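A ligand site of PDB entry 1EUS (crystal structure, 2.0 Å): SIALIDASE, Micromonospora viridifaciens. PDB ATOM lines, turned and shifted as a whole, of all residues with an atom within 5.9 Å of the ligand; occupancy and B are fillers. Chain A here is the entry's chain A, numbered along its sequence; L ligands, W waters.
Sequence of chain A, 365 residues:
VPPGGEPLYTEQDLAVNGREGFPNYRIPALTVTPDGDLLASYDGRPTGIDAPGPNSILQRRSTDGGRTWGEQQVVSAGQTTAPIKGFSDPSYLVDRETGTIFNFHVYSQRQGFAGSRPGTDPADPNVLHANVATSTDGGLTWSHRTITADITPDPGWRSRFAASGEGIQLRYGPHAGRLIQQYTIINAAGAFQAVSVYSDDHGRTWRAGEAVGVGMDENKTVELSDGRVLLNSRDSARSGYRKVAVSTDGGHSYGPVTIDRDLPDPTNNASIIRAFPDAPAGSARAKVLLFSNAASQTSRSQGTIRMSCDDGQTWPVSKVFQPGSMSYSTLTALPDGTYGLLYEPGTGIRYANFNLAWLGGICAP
The guanidinium group of Arg 234 lies within salt-bridge range of an oxygen (O2) of the ligand, at 3.2 Å.
O4 of the ligand sits close to OH of Tyr 328 (3.0 Å).
The guanidinium group of Arg 26 lies within salt-bridge range of an oxygen (O1) of the ligand (2.7 Å).
NH1 of Arg 300 lies within salt-bridge range of O1 of the ligand (2.8 Å).
An oxygen (O3) of the ligand lies within hydrogen-bond range of the side-chain carboxylate of Asp 89 (2.7 Å).
An oxygen (O6) of the ligand lies within hydrogen-bond range of the side-chain carboxylate (OD1) of Asp 217.
An oxygen (O3) of the ligand sits at hydrogen-bond distance from the guanidinium group (NH2) of Arg 45, at 3.0 Å.
OD1 of Asp 50 lies within hydrogen-bond range of O3 of the ligand, 2.7 Å away.
Residues that only touch the ligand: Ile 27 (3.5 Å), Phe 113 (3.5 Å), Phe 161 (3.5 Å), Phe 192 (3.7 Å) and Glu 218 (3.8 Å).
Hydrophobic or aromatic side chains that line the ligand: Ile 27, Phe 113, Phe 161, Phe 192 and Tyr 328.
Of the 22 residues printed, 13 come within 4 Å of the ligand.
The nearest printed residue that does not touch the ligand is Val 106 (4.2 Å).
Water W3 lies within hydrogen-bond range of an oxygen (O8) of the ligand, the backbone carbonyl oxygen of Ala 51 and the backbone NH of Phe 113.
Water W1 lies within hydrogen-bond range of the side-chain carboxylate (OD1) of Asp 89 (2.9 Å), the backbone NH (N) of Ala 51 (3.1 Å), an oxygen (O3) of the ligand (3.2 Å) and the guanidinium group (NH2) of Arg 45 (3.4 Å).
OD1 of Asp 89 is in salt-bridge range of NH2 of Arg 45, 3.7 Å away.
The backbone NH (N) of Asp 89 lies within hydrogen-bond range of the side-chain carboxylate (OD1) of Asp 43 (2.9 Å).
The side-chain carboxylate of Glu 218 sits at hydrogen-bond distance from the side-chain hydroxyl of Tyr 328 (2.6 Å).
The guanidinium group (NH2) of Arg 234 lies within salt-bridge range of the side-chain carboxylate (OE1) of Glu 218 (2.8 Å).
The backbone NH (N) of Tyr 328 lies within hydrogen-bond range of the side-chain carboxylate (OE1) of Glu 344 (2.9 Å).
NE of Arg 300 sits close to ND2 of Asn 268 (3.3 Å).
The backbone NH (N) of Asp 43 is in hydrogen-bond range of the backbone carbonyl oxygen (O) of Arg 26 (2.7 Å).
The side-chain carboxylate (OD1) of Asp 217 lies within salt-bridge range of the guanidinium group (NE) of Arg 234, at 3.7 Å.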
ATOM      1  N   ARG A  26      -7.643 -14.592  -0.370  1.00  0.00           N
ATOM      2  CA  ARG A  26      -8.891 -14.023  -0.890  1.00  0.00           C
ATOM      3  C   ARG A  26      -9.362 -14.744  -2.135  1.00  0.00           C
ATOM      4  O   ARG A  26      -8.597 -15.446  -2.777  1.00  0.00           O
ATOM      5  CB  ARG A  26      -8.739 -12.532  -1.274  1.00  0.00           C
ATOM      6  CG  ARG A  26      -8.974 -11.499  -0.156  1.00  0.00           C
ATOM      7  CD  ARG A  26      -9.477 -10.167  -0.730  1.00  0.00           C
ATOM      8  NE  ARG A  26     -10.890 -10.253  -1.145  1.00  0.00           N
ATOM      9  CZ  ARG A  26     -11.517  -9.382  -1.942  1.00  0.00           C
ATOM     10  NH1 ARG A  26     -10.879  -8.319  -2.445  1.00  0.00           N
ATOM     11  NH2 ARG A  26     -12.798  -9.568  -2.217  1.00  0.00           N
ATOM     12  N   ILE A  27     -10.602 -14.436  -2.527  1.00  0.00           N
ATOM     13  CA  ILE A  27     -11.256 -14.927  -3.748  1.00  0.00           C
ATOM     14  C   ILE A  27     -11.555 -16.410  -3.826  1.00  0.00           C
ATOM     15  O   ILE A  27     -10.762 -17.182  -4.335  1.00  0.00           O
ATOM     16  CB  ILE A  27     -10.458 -14.511  -5.025  1.00  0.00           C
ATOM     17  CG1 ILE A  27      -9.830 -13.126  -4.891  1.00  0.00           C
ATOM     18  CG2 ILE A  27     -11.404 -14.516  -6.202  1.00  0.00           C
ATOM     19  CD1 ILE A  27     -10.825 -11.996  -4.632  1.00  0.00           C
ATOM     20  N   ASP A  43      -6.965 -17.321  -3.793  1.00  0.00           N
ATOM     21  CA  ASP A  43      -5.698 -16.609  -3.964  1.00  0.00           C
ATOM     22  C   ASP A  43      -4.835 -16.676  -2.689  1.00  0.00           C
ATOM     23  O   ASP A  43      -5.351 -16.583  -1.566  1.00  0.00           O
ATOM     24  CB  ASP A  43      -5.943 -15.114  -4.202  1.00  0.00           C
ATOM     25  CG  ASP A  43      -6.278 -14.739  -5.631  1.00  0.00           C
ATOM     26  OD1 ASP A  43      -6.775 -15.579  -6.415  1.00  0.00           O
ATOM     27  OD2 ASP A  43      -6.079 -13.573  -5.960  1.00  0.00           O
ATOM     28  N   ARG A  45      -1.977 -14.375  -1.420  1.00  0.00           N
ATOM     29  CA  ARG A  45      -1.476 -13.065  -1.799  1.00  0.00           C
ATOM     30  C   ARG A  45      -0.321 -12.549  -0.942  1.00  0.00           C
ATOM     31  O   ARG A  45      -0.541 -12.005   0.132  1.00  0.00           O
ATOM     32  CB  ARG A  45      -2.629 -12.049  -1.770  1.00  0.00           C
ATOM     33  CG  ARG A  45      -3.781 -12.426  -2.689  1.00  0.00           C
ATOM     34  CD  ARG A  45      -4.927 -11.417  -2.664  1.00  0.00           C
ATOM     35  NE  ARG A  45      -5.708 -11.526  -3.894  1.00  0.00           N
ATOM     36  CZ  ARG A  45      -6.600 -10.638  -4.331  1.00  0.00           C
ATOM     37  NH1 ARG A  45      -6.879  -9.548  -3.626  1.00  0.00           N
ATOM     38  NH2 ARG A  45      -7.204 -10.858  -5.509  1.00  0.00           N
ATOM     39  N   ASP A  50      -4.643  -7.203  -5.313  1.00  0.00           N
ATOM     40  CA  ASP A  50      -5.146  -7.836  -6.547  1.00  0.00           C
ATOM     41  C   ASP A  50      -4.048  -7.807  -7.610  1.00  0.00           C
ATOM     42  O   ASP A  50      -2.952  -7.259  -7.370  1.00  0.00           O
ATOM     43  CB  ASP A  50      -6.377  -7.080  -7.070  1.00  0.00           C
ATOM     44  CG  ASP A  50      -7.546  -7.081  -6.096  1.00  0.00           C
ATOM     45  OD1 ASP A  50      -7.996  -8.171  -5.705  1.00  0.00           O
ATOM     46  OD2 ASP A  50      -8.026  -5.995  -5.739  1.00  0.00           O
ATOM     47  N   ALA A  51      -4.315  -8.387  -8.781  1.00  0.00           N
ATOM     48  CA  ALA A  51      -3.355  -8.390  -9.876  1.00  0.00           C
ATOM     49  C   ALA A  51      -3.038  -6.896 -10.085  1.00  0.00           C
ATOM     50  O   ALA A  51      -3.940  -6.055  -9.971  1.00  0.00           O
ATOM     51  CB  ALA A  51      -3.984  -8.984 -11.128  1.00  0.00           C
ATOM     52  N   SER A  88      -4.350 -15.014 -10.204  1.00  0.00           N
ATOM     53  CA  SER A  88      -5.478 -14.657  -9.341  1.00  0.00           C
ATOM     54  C   SER A  88      -6.863 -14.929  -9.874  1.00  0.00           C
ATOM     55  O   SER A  88      -7.053 -15.033 -11.078  1.00  0.00           O
ATOM     56  CB  SER A  88      -5.495 -13.130  -9.101  1.00  0.00           C
ATOM     57  OG  SER A  88      -4.472 -12.719  -8.254  1.00  0.00           O
ATOM     58  N   ASP A  89      -7.847 -14.766  -8.973  1.00  0.00           N
ATOM     59  CA  ASP A  89      -9.280 -14.916  -9.254  1.00  0.00           C
ATOM     60  C   ASP A  89      -9.646 -16.205  -9.929  1.00  0.00           C
ATOM     61  O   ASP A  89      -9.901 -16.226 -11.127  1.00  0.00           O
ATOM     62  CB  ASP A  89      -9.787 -13.741 -10.098  1.00  0.00           C
ATOM     63  CG  ASP A  89      -9.866 -12.432  -9.320  1.00  0.00           C
ATOM     64  OD1 ASP A  89      -8.926 -12.101  -8.575  1.00  0.00           O
ATOM     65  OD2 ASP A  89     -10.885 -11.736  -9.444  1.00  0.00           O
ATOM     66  N   VAL A 106      -6.500 -15.360 -13.975  1.00  0.00           N
ATOM     67  CA  VAL A 106      -5.702 -14.302 -14.510  1.00  0.00           C
ATOM     68  C   VAL A 106      -4.224 -14.709 -14.508  1.00  0.00           C
ATOM     69  O   VAL A 106      -3.813 -15.512 -13.676  1.00  0.00           O
ATOM     70  CB  VAL A 106      -5.915 -13.075 -13.576  1.00  0.00           C
ATOM     71  CG1 VAL A 106      -4.670 -12.255 -13.385  1.00  0.00           C
ATOM     72  CG2 VAL A 106      -7.081 -12.275 -14.033  1.00  0.00           C
ATOM     73  N   PHE A 113      -6.139  -5.437 -14.155  1.00  0.00           N
ATOM     74  CA  PHE A 113      -7.330  -5.245 -14.954  1.00  0.00           C
ATOM     75  C   PHE A 113      -7.493  -3.850 -15.528  1.00  0.00           C
ATOM     76  O   PHE A 113      -7.668  -3.695 -16.749  1.00  0.00           O
ATOM     77  CB  PHE A 113      -8.574  -5.639 -14.129  1.00  0.00           C
ATOM     78  CG  PHE A 113      -9.893  -5.459 -14.855  1.00  0.00           C
ATOM     79  CD1 PHE A 113     -10.196  -6.196 -16.003  1.00  0.00           C
ATOM     80  CD2 PHE A 113     -10.858  -4.589 -14.356  1.00  0.00           C
ATOM     81  CE1 PHE A 113     -11.448  -6.075 -16.627  1.00  0.00           C
ATOM     82  CE2 PHE A 113     -12.096  -4.459 -14.964  1.00  0.00           C
ATOM     83  CZ  PHE A 113     -12.394  -5.195 -16.104  1.00  0.00           C
ATOM     84  N   LEU A 128      -3.154  -8.165 -19.411  1.00  0.00           N
ATOM     85  CA  LEU A 128      -3.655  -9.067 -18.381  1.00  0.00           C
ATOM     86  C   LEU A 128      -4.152 -10.277 -19.184  1.00  0.00           C
ATOM     87  O   LEU A 128      -5.131 -10.192 -19.926  1.00  0.00           O
ATOM     88  CB  LEU A 128      -4.835  -8.442 -17.603  1.00  0.00           C
ATOM     89  CG  LEU A 128      -5.337  -9.292 -16.429  1.00  0.00           C
ATOM     90  CD1 LEU A 128      -4.236  -9.447 -15.377  1.00  0.00           C
ATOM     91  CD2 LEU A 128      -6.575  -8.678 -15.789  1.00  0.00           C
ATOM     92  N   PHE A 161     -11.048 -10.608 -17.482  1.00  0.00           N
ATOM     93  CA  PHE A 161     -10.827 -11.504 -16.355  1.00  0.00           C
ATOM     94  C   PHE A 161     -12.060 -12.349 -16.107  1.00  0.00           C
ATOM     95  O   PHE A 161     -13.187 -11.876 -16.215  1.00  0.00           O
ATOM     96  CB  PHE A 161     -10.297 -10.775 -15.083  1.00  0.00           C
ATOM     97  CG  PHE A 161     -11.347 -10.070 -14.226  1.00  0.00           C
ATOM     98  CD1 PHE A 161     -11.828  -8.806 -14.564  1.00  0.00           C
ATOM     99  CD2 PHE A 161     -11.726 -10.604 -12.991  1.00  0.00           C
ATOM    100  CE1 PHE A 161     -12.660  -8.086 -13.679  1.00  0.00           C
ATOM    101  CE2 PHE A 161     -12.563  -9.884 -12.115  1.00  0.00           C
ATOM    102  CZ  PHE A 161     -13.029  -8.632 -12.459  1.00  0.00           C
ATOM    103  N   PHE A 192     -17.010  -1.162 -19.295  1.00  0.00           N
ATOM    104  CA  PHE A 192     -16.942  -2.486 -18.668  1.00  0.00           C
ATOM    105  C   PHE A 192     -18.131  -3.280 -19.209  1.00  0.00           C
ATOM    106  O   PHE A 192     -19.281  -2.884 -19.014  1.00  0.00           O
ATOM    107  CB  PHE A 192     -17.118  -2.400 -17.142  1.00  0.00           C
ATOM    108  CG  PHE A 192     -15.880  -1.985 -16.377  1.00  0.00           C
ATOM    109  CD1 PHE A 192     -14.908  -1.187 -16.964  1.00  0.00           C
ATOM    110  CD2 PHE A 192     -15.700  -2.385 -15.061  1.00  0.00           C
ATOM    111  CE1 PHE A 192     -13.800  -0.803 -16.246  1.00  0.00           C
ATOM    112  CE2 PHE A 192     -14.579  -1.999 -14.349  1.00  0.00           C
ATOM    113  CZ  PHE A 192     -13.629  -1.211 -14.936  1.00  0.00           C
ATOM    114  N   ASP A 217     -19.573  -5.868 -14.586  1.00  0.00           N
ATOM    115  CA  ASP A 217     -18.446  -6.340 -13.778  1.00  0.00           C
ATOM    116  C   ASP A 217     -18.563  -7.848 -13.621  1.00  0.00           C
ATOM    117  O   ASP A 217     -19.219  -8.501 -14.457  1.00  0.00           O
ATOM    118  CB  ASP A 217     -18.440  -5.653 -12.407  1.00  0.00           C
ATOM    119  CG  ASP A 217     -17.035  -5.435 -11.882  1.00  0.00           C
ATOM    120  OD1 ASP A 217     -16.296  -6.420 -11.757  1.00  0.00           O
ATOM    121  OD2 ASP A 217     -16.682  -4.272 -11.618  1.00  0.00           O
ATOM    122  N   GLU A 218     -17.967  -8.418 -12.565  1.00  0.00           N
ATOM    123  CA  GLU A 218     -18.024  -9.862 -12.328  1.00  0.00           C
ATOM    124  C   GLU A 218     -19.471 -10.282 -12.481  1.00  0.00           C
ATOM    125  O   GLU A 218     -20.376  -9.707 -11.856  1.00  0.00           O
ATOM    126  CB  GLU A 218     -17.551 -10.224 -10.920  1.00  0.00           C
ATOM    127  CG  GLU A 218     -16.086  -9.931 -10.704  1.00  0.00           C
ATOM    128  CD  GLU A 218     -15.753  -9.728  -9.240  1.00  0.00           C
ATOM    129  OE1 GLU A 218     -16.644  -9.240  -8.518  1.00  0.00           O
ATOM    130  OE2 GLU A 218     -14.616 -10.038  -8.832  1.00  0.00           O
ATOM    131  N   ARG A 234     -22.541  -7.904 -11.191  1.00  0.00           N
ATOM    132  CA  ARG A 234     -22.146  -6.892 -10.220  1.00  0.00           C
ATOM    133  C   ARG A 234     -22.267  -5.618 -11.087  1.00  0.00           C
ATOM    134  O   ARG A 234     -21.948  -5.644 -12.283  1.00  0.00           O
ATOM    135  CB  ARG A 234     -20.661  -7.038  -9.797  1.00  0.00           C
ATOM    136  CG  ARG A 234     -20.183  -5.847  -8.939  1.00  0.00           C
ATOM    137  CD  ARG A 234     -18.731  -5.445  -9.076  1.00  0.00           C
ATOM    138  NE  ARG A 234     -17.872  -6.360  -8.356  1.00  0.00           N
ATOM    139  CZ  ARG A 234     -16.753  -6.037  -7.686  1.00  0.00           C
ATOM    140  NH1 ARG A 234     -16.312  -4.783  -7.634  1.00  0.00           N
ATOM    141  NH2 ARG A 234     -16.098  -6.979  -7.033  1.00  0.00           N
ATOM    142  N   SER A 236     -20.826  -2.126 -11.856  1.00  0.00           N
ATOM    143  CA  SER A 236     -19.687  -1.224 -11.595  1.00  0.00           C
ATOM    144  C   SER A 236     -20.118   0.243 -11.553  1.00  0.00           C
ATOM    145  O   SER A 236     -19.338   1.113 -11.173  1.00  0.00           O
ATOM    146  CB  SER A 236     -18.547  -1.432 -12.614  1.00  0.00           C
ATOM    147  OG  SER A 236     -18.971  -1.195 -13.929  1.00  0.00           O
ATOM    148  N   THR A 267     -22.027  -3.620  -4.713  1.00  0.00           N
ATOM    149  CA  THR A 267     -21.021  -3.696  -5.784  1.00  0.00           C
ATOM    150  C   THR A 267     -19.956  -4.647  -5.273  1.00  0.00           C
ATOM    151  O   THR A 267     -18.900  -4.256  -4.774  1.00  0.00           O
ATOM    152  CB  THR A 267     -20.451  -2.311  -6.177  1.00  0.00           C
ATOM    153  OG1 THR A 267     -21.539  -1.513  -6.671  1.00  0.00           O
ATOM    154  CG2 THR A 267     -19.431  -2.433  -7.286  1.00  0.00           C
ATOM    155  N   ASN A 268     -20.265  -5.915  -5.432  1.00  0.00           N
ATOM    156  CA  ASN A 268     -19.447  -6.995  -4.897  1.00  0.00           C
ATOM    157  C   ASN A 268     -19.861  -8.258  -5.694  1.00  0.00           C
ATOM    158  O   ASN A 268     -20.858  -8.240  -6.414  1.00  0.00           O
ATOM    159  CB  ASN A 268     -19.831  -7.030  -3.400  1.00  0.00           C
ATOM    160  CG  ASN A 268     -19.235  -8.213  -2.621  1.00  0.00           C
ATOM    161  OD1 ASN A 268     -19.929  -8.835  -1.830  1.00  0.00           O
ATOM    162  ND2 ASN A 268     -17.931  -8.446  -2.774  1.00  0.00           N
ATOM    163  N   ARG A 300     -19.901  -4.334   2.530  1.00  0.00           N
ATOM    164  CA  ARG A 300     -19.831  -5.751   2.238  1.00  0.00           C
ATOM    165  C   ARG A 300     -20.099  -6.514   3.529  1.00  0.00           C
ATOM    166  O   ARG A 300     -19.179  -6.920   4.245  1.00  0.00           O
ATOM    167  CB  ARG A 300     -18.475  -6.106   1.632  1.00  0.00           C
ATOM    168  CG  ARG A 300     -18.277  -5.444   0.279  1.00  0.00           C
ATOM    169  CD  ARG A 300     -17.057  -5.950  -0.445  1.00  0.00           C
ATOM    170  NE  ARG A 300     -16.980  -5.426  -1.813  1.00  0.00           N
ATOM    171  CZ  ARG A 300     -15.997  -5.683  -2.666  1.00  0.00           C
ATOM    172  NH1 ARG A 300     -14.977  -6.450  -2.317  1.00  0.00           N
ATOM    173  NH2 ARG A 300     -16.055  -5.197  -3.900  1.00  0.00           N
ATOM    174  N   TYR A 328     -16.826 -11.811  -0.915  1.00  0.00           N
ATOM    175  CA  TYR A 328     -17.159 -12.754  -1.996  1.00  0.00           C
ATOM    176  C   TYR A 328     -17.700 -14.084  -1.430  1.00  0.00           C
ATOM    177  O   TYR A 328     -17.257 -14.547  -0.360  1.00  0.00           O
ATOM    178  CB  TYR A 328     -15.935 -13.055  -2.874  1.00  0.00           C
ATOM    179  CG  TYR A 328     -15.493 -11.949  -3.829  1.00  0.00           C
ATOM    180  CD1 TYR A 328     -15.836 -10.604  -3.614  1.00  0.00           C
ATOM    181  CD2 TYR A 328     -14.714 -12.241  -4.948  1.00  0.00           C
ATOM    182  CE1 TYR A 328     -15.430  -9.584  -4.492  1.00  0.00           C
ATOM    183  CE2 TYR A 328     -14.300 -11.220  -5.841  1.00  0.00           C
ATOM    184  CZ  TYR A 328     -14.667  -9.900  -5.603  1.00  0.00           C
ATOM    185  OH  TYR A 328     -14.304  -8.915  -6.481  1.00  0.00           O
ATOM    186  N   GLU A 344     -15.826 -15.135   2.127  1.00  0.00           N
ATOM    187  CA  GLU A 344     -14.802 -14.295   2.735  1.00  0.00           C
ATOM    188  C   GLU A 344     -15.334 -13.535   3.940  1.00  0.00           C
ATOM    189  O   GLU A 344     -16.103 -12.581   3.775  1.00  0.00           O
ATOM    190  CB  GLU A 344     -14.264 -13.261   1.759  1.00  0.00           C
ATOM    191  CG  GLU A 344     -13.627 -13.819   0.507  1.00  0.00           C
ATOM    192  CD  GLU A 344     -13.192 -12.707  -0.444  1.00  0.00           C
ATOM    193  OE1 GLU A 344     -13.962 -11.751  -0.675  1.00  0.00           O
ATOM    194  OE2 GLU A 344     -12.067 -12.775  -0.961  1.00  0.00           O
HETATM  195  C1  LIG L   1     -12.827  -6.740  -5.153  1.00  0.00           C
HETATM  196  C2  LIG L   1     -12.086  -7.252  -6.257  1.00  0.00           C
HETATM  197  C3  LIG L   1     -11.285  -8.373  -6.079  1.00  0.00           C
HETATM  198  C4  LIG L   1     -10.786  -9.129  -7.335  1.00  0.00           C
HETATM  199  C5  LIG L   1     -10.528  -8.149  -8.529  1.00  0.00           C
HETATM  200  C6  LIG L   1     -11.835  -7.374  -8.828  1.00  0.00           C
HETATM  201  C7  LIG L   1     -11.833  -6.171  -9.840  1.00  0.00           C
HETATM  202  C8  LIG L   1     -13.221  -5.408  -9.656  1.00  0.00           C
HETATM  203  C9  LIG L   1     -13.498  -4.078 -10.516  1.00  0.00           C
HETATM  204  C10 LIG L   1      -9.151  -8.373 -10.517  1.00  0.00           C
HETATM  205  C11 LIG L   1      -8.618  -9.155 -11.710  1.00  0.00           C
HETATM  206  N1  LIG L   1     -10.052  -8.896  -9.696  1.00  0.00           N
HETATM  207  O1  LIG L   1     -12.857  -7.278  -4.018  1.00  0.00           O
HETATM  208  O2  LIG L   1     -13.593  -5.782  -5.408  1.00  0.00           O
HETATM  209  O3  LIG L   1      -9.583  -9.874  -7.109  1.00  0.00           O
HETATM  210  O4  LIG L   1     -12.359  -6.836  -7.563  1.00  0.00           O
HETATM  211  O5  LIG L   1     -10.722  -5.394  -9.561  1.00  0.00           O
HETATM  212  O6  LIG L   1     -14.216  -6.357 -10.062  1.00  0.00           O
HETATM  213  O7  LIG L   1     -13.583  -4.409 -11.773  1.00  0.00           O
HETATM  214  O8  LIG L   1      -8.742  -7.205 -10.380  1.00  0.00           O
HETATM  215  O   HOH W   1      -6.902 -10.058  -8.805  1.00  0.00           O
HETATM  216  O   HOH W   2      -9.611  -2.785 -10.327  1.00  0.00           O
HETATM  217  O   HOH W   3      -6.409  -6.054 -11.336  1.00  0.00           O
HETATM  218  O   HOH W   4     -10.842  -3.726  -7.189  1.00  0.00           O
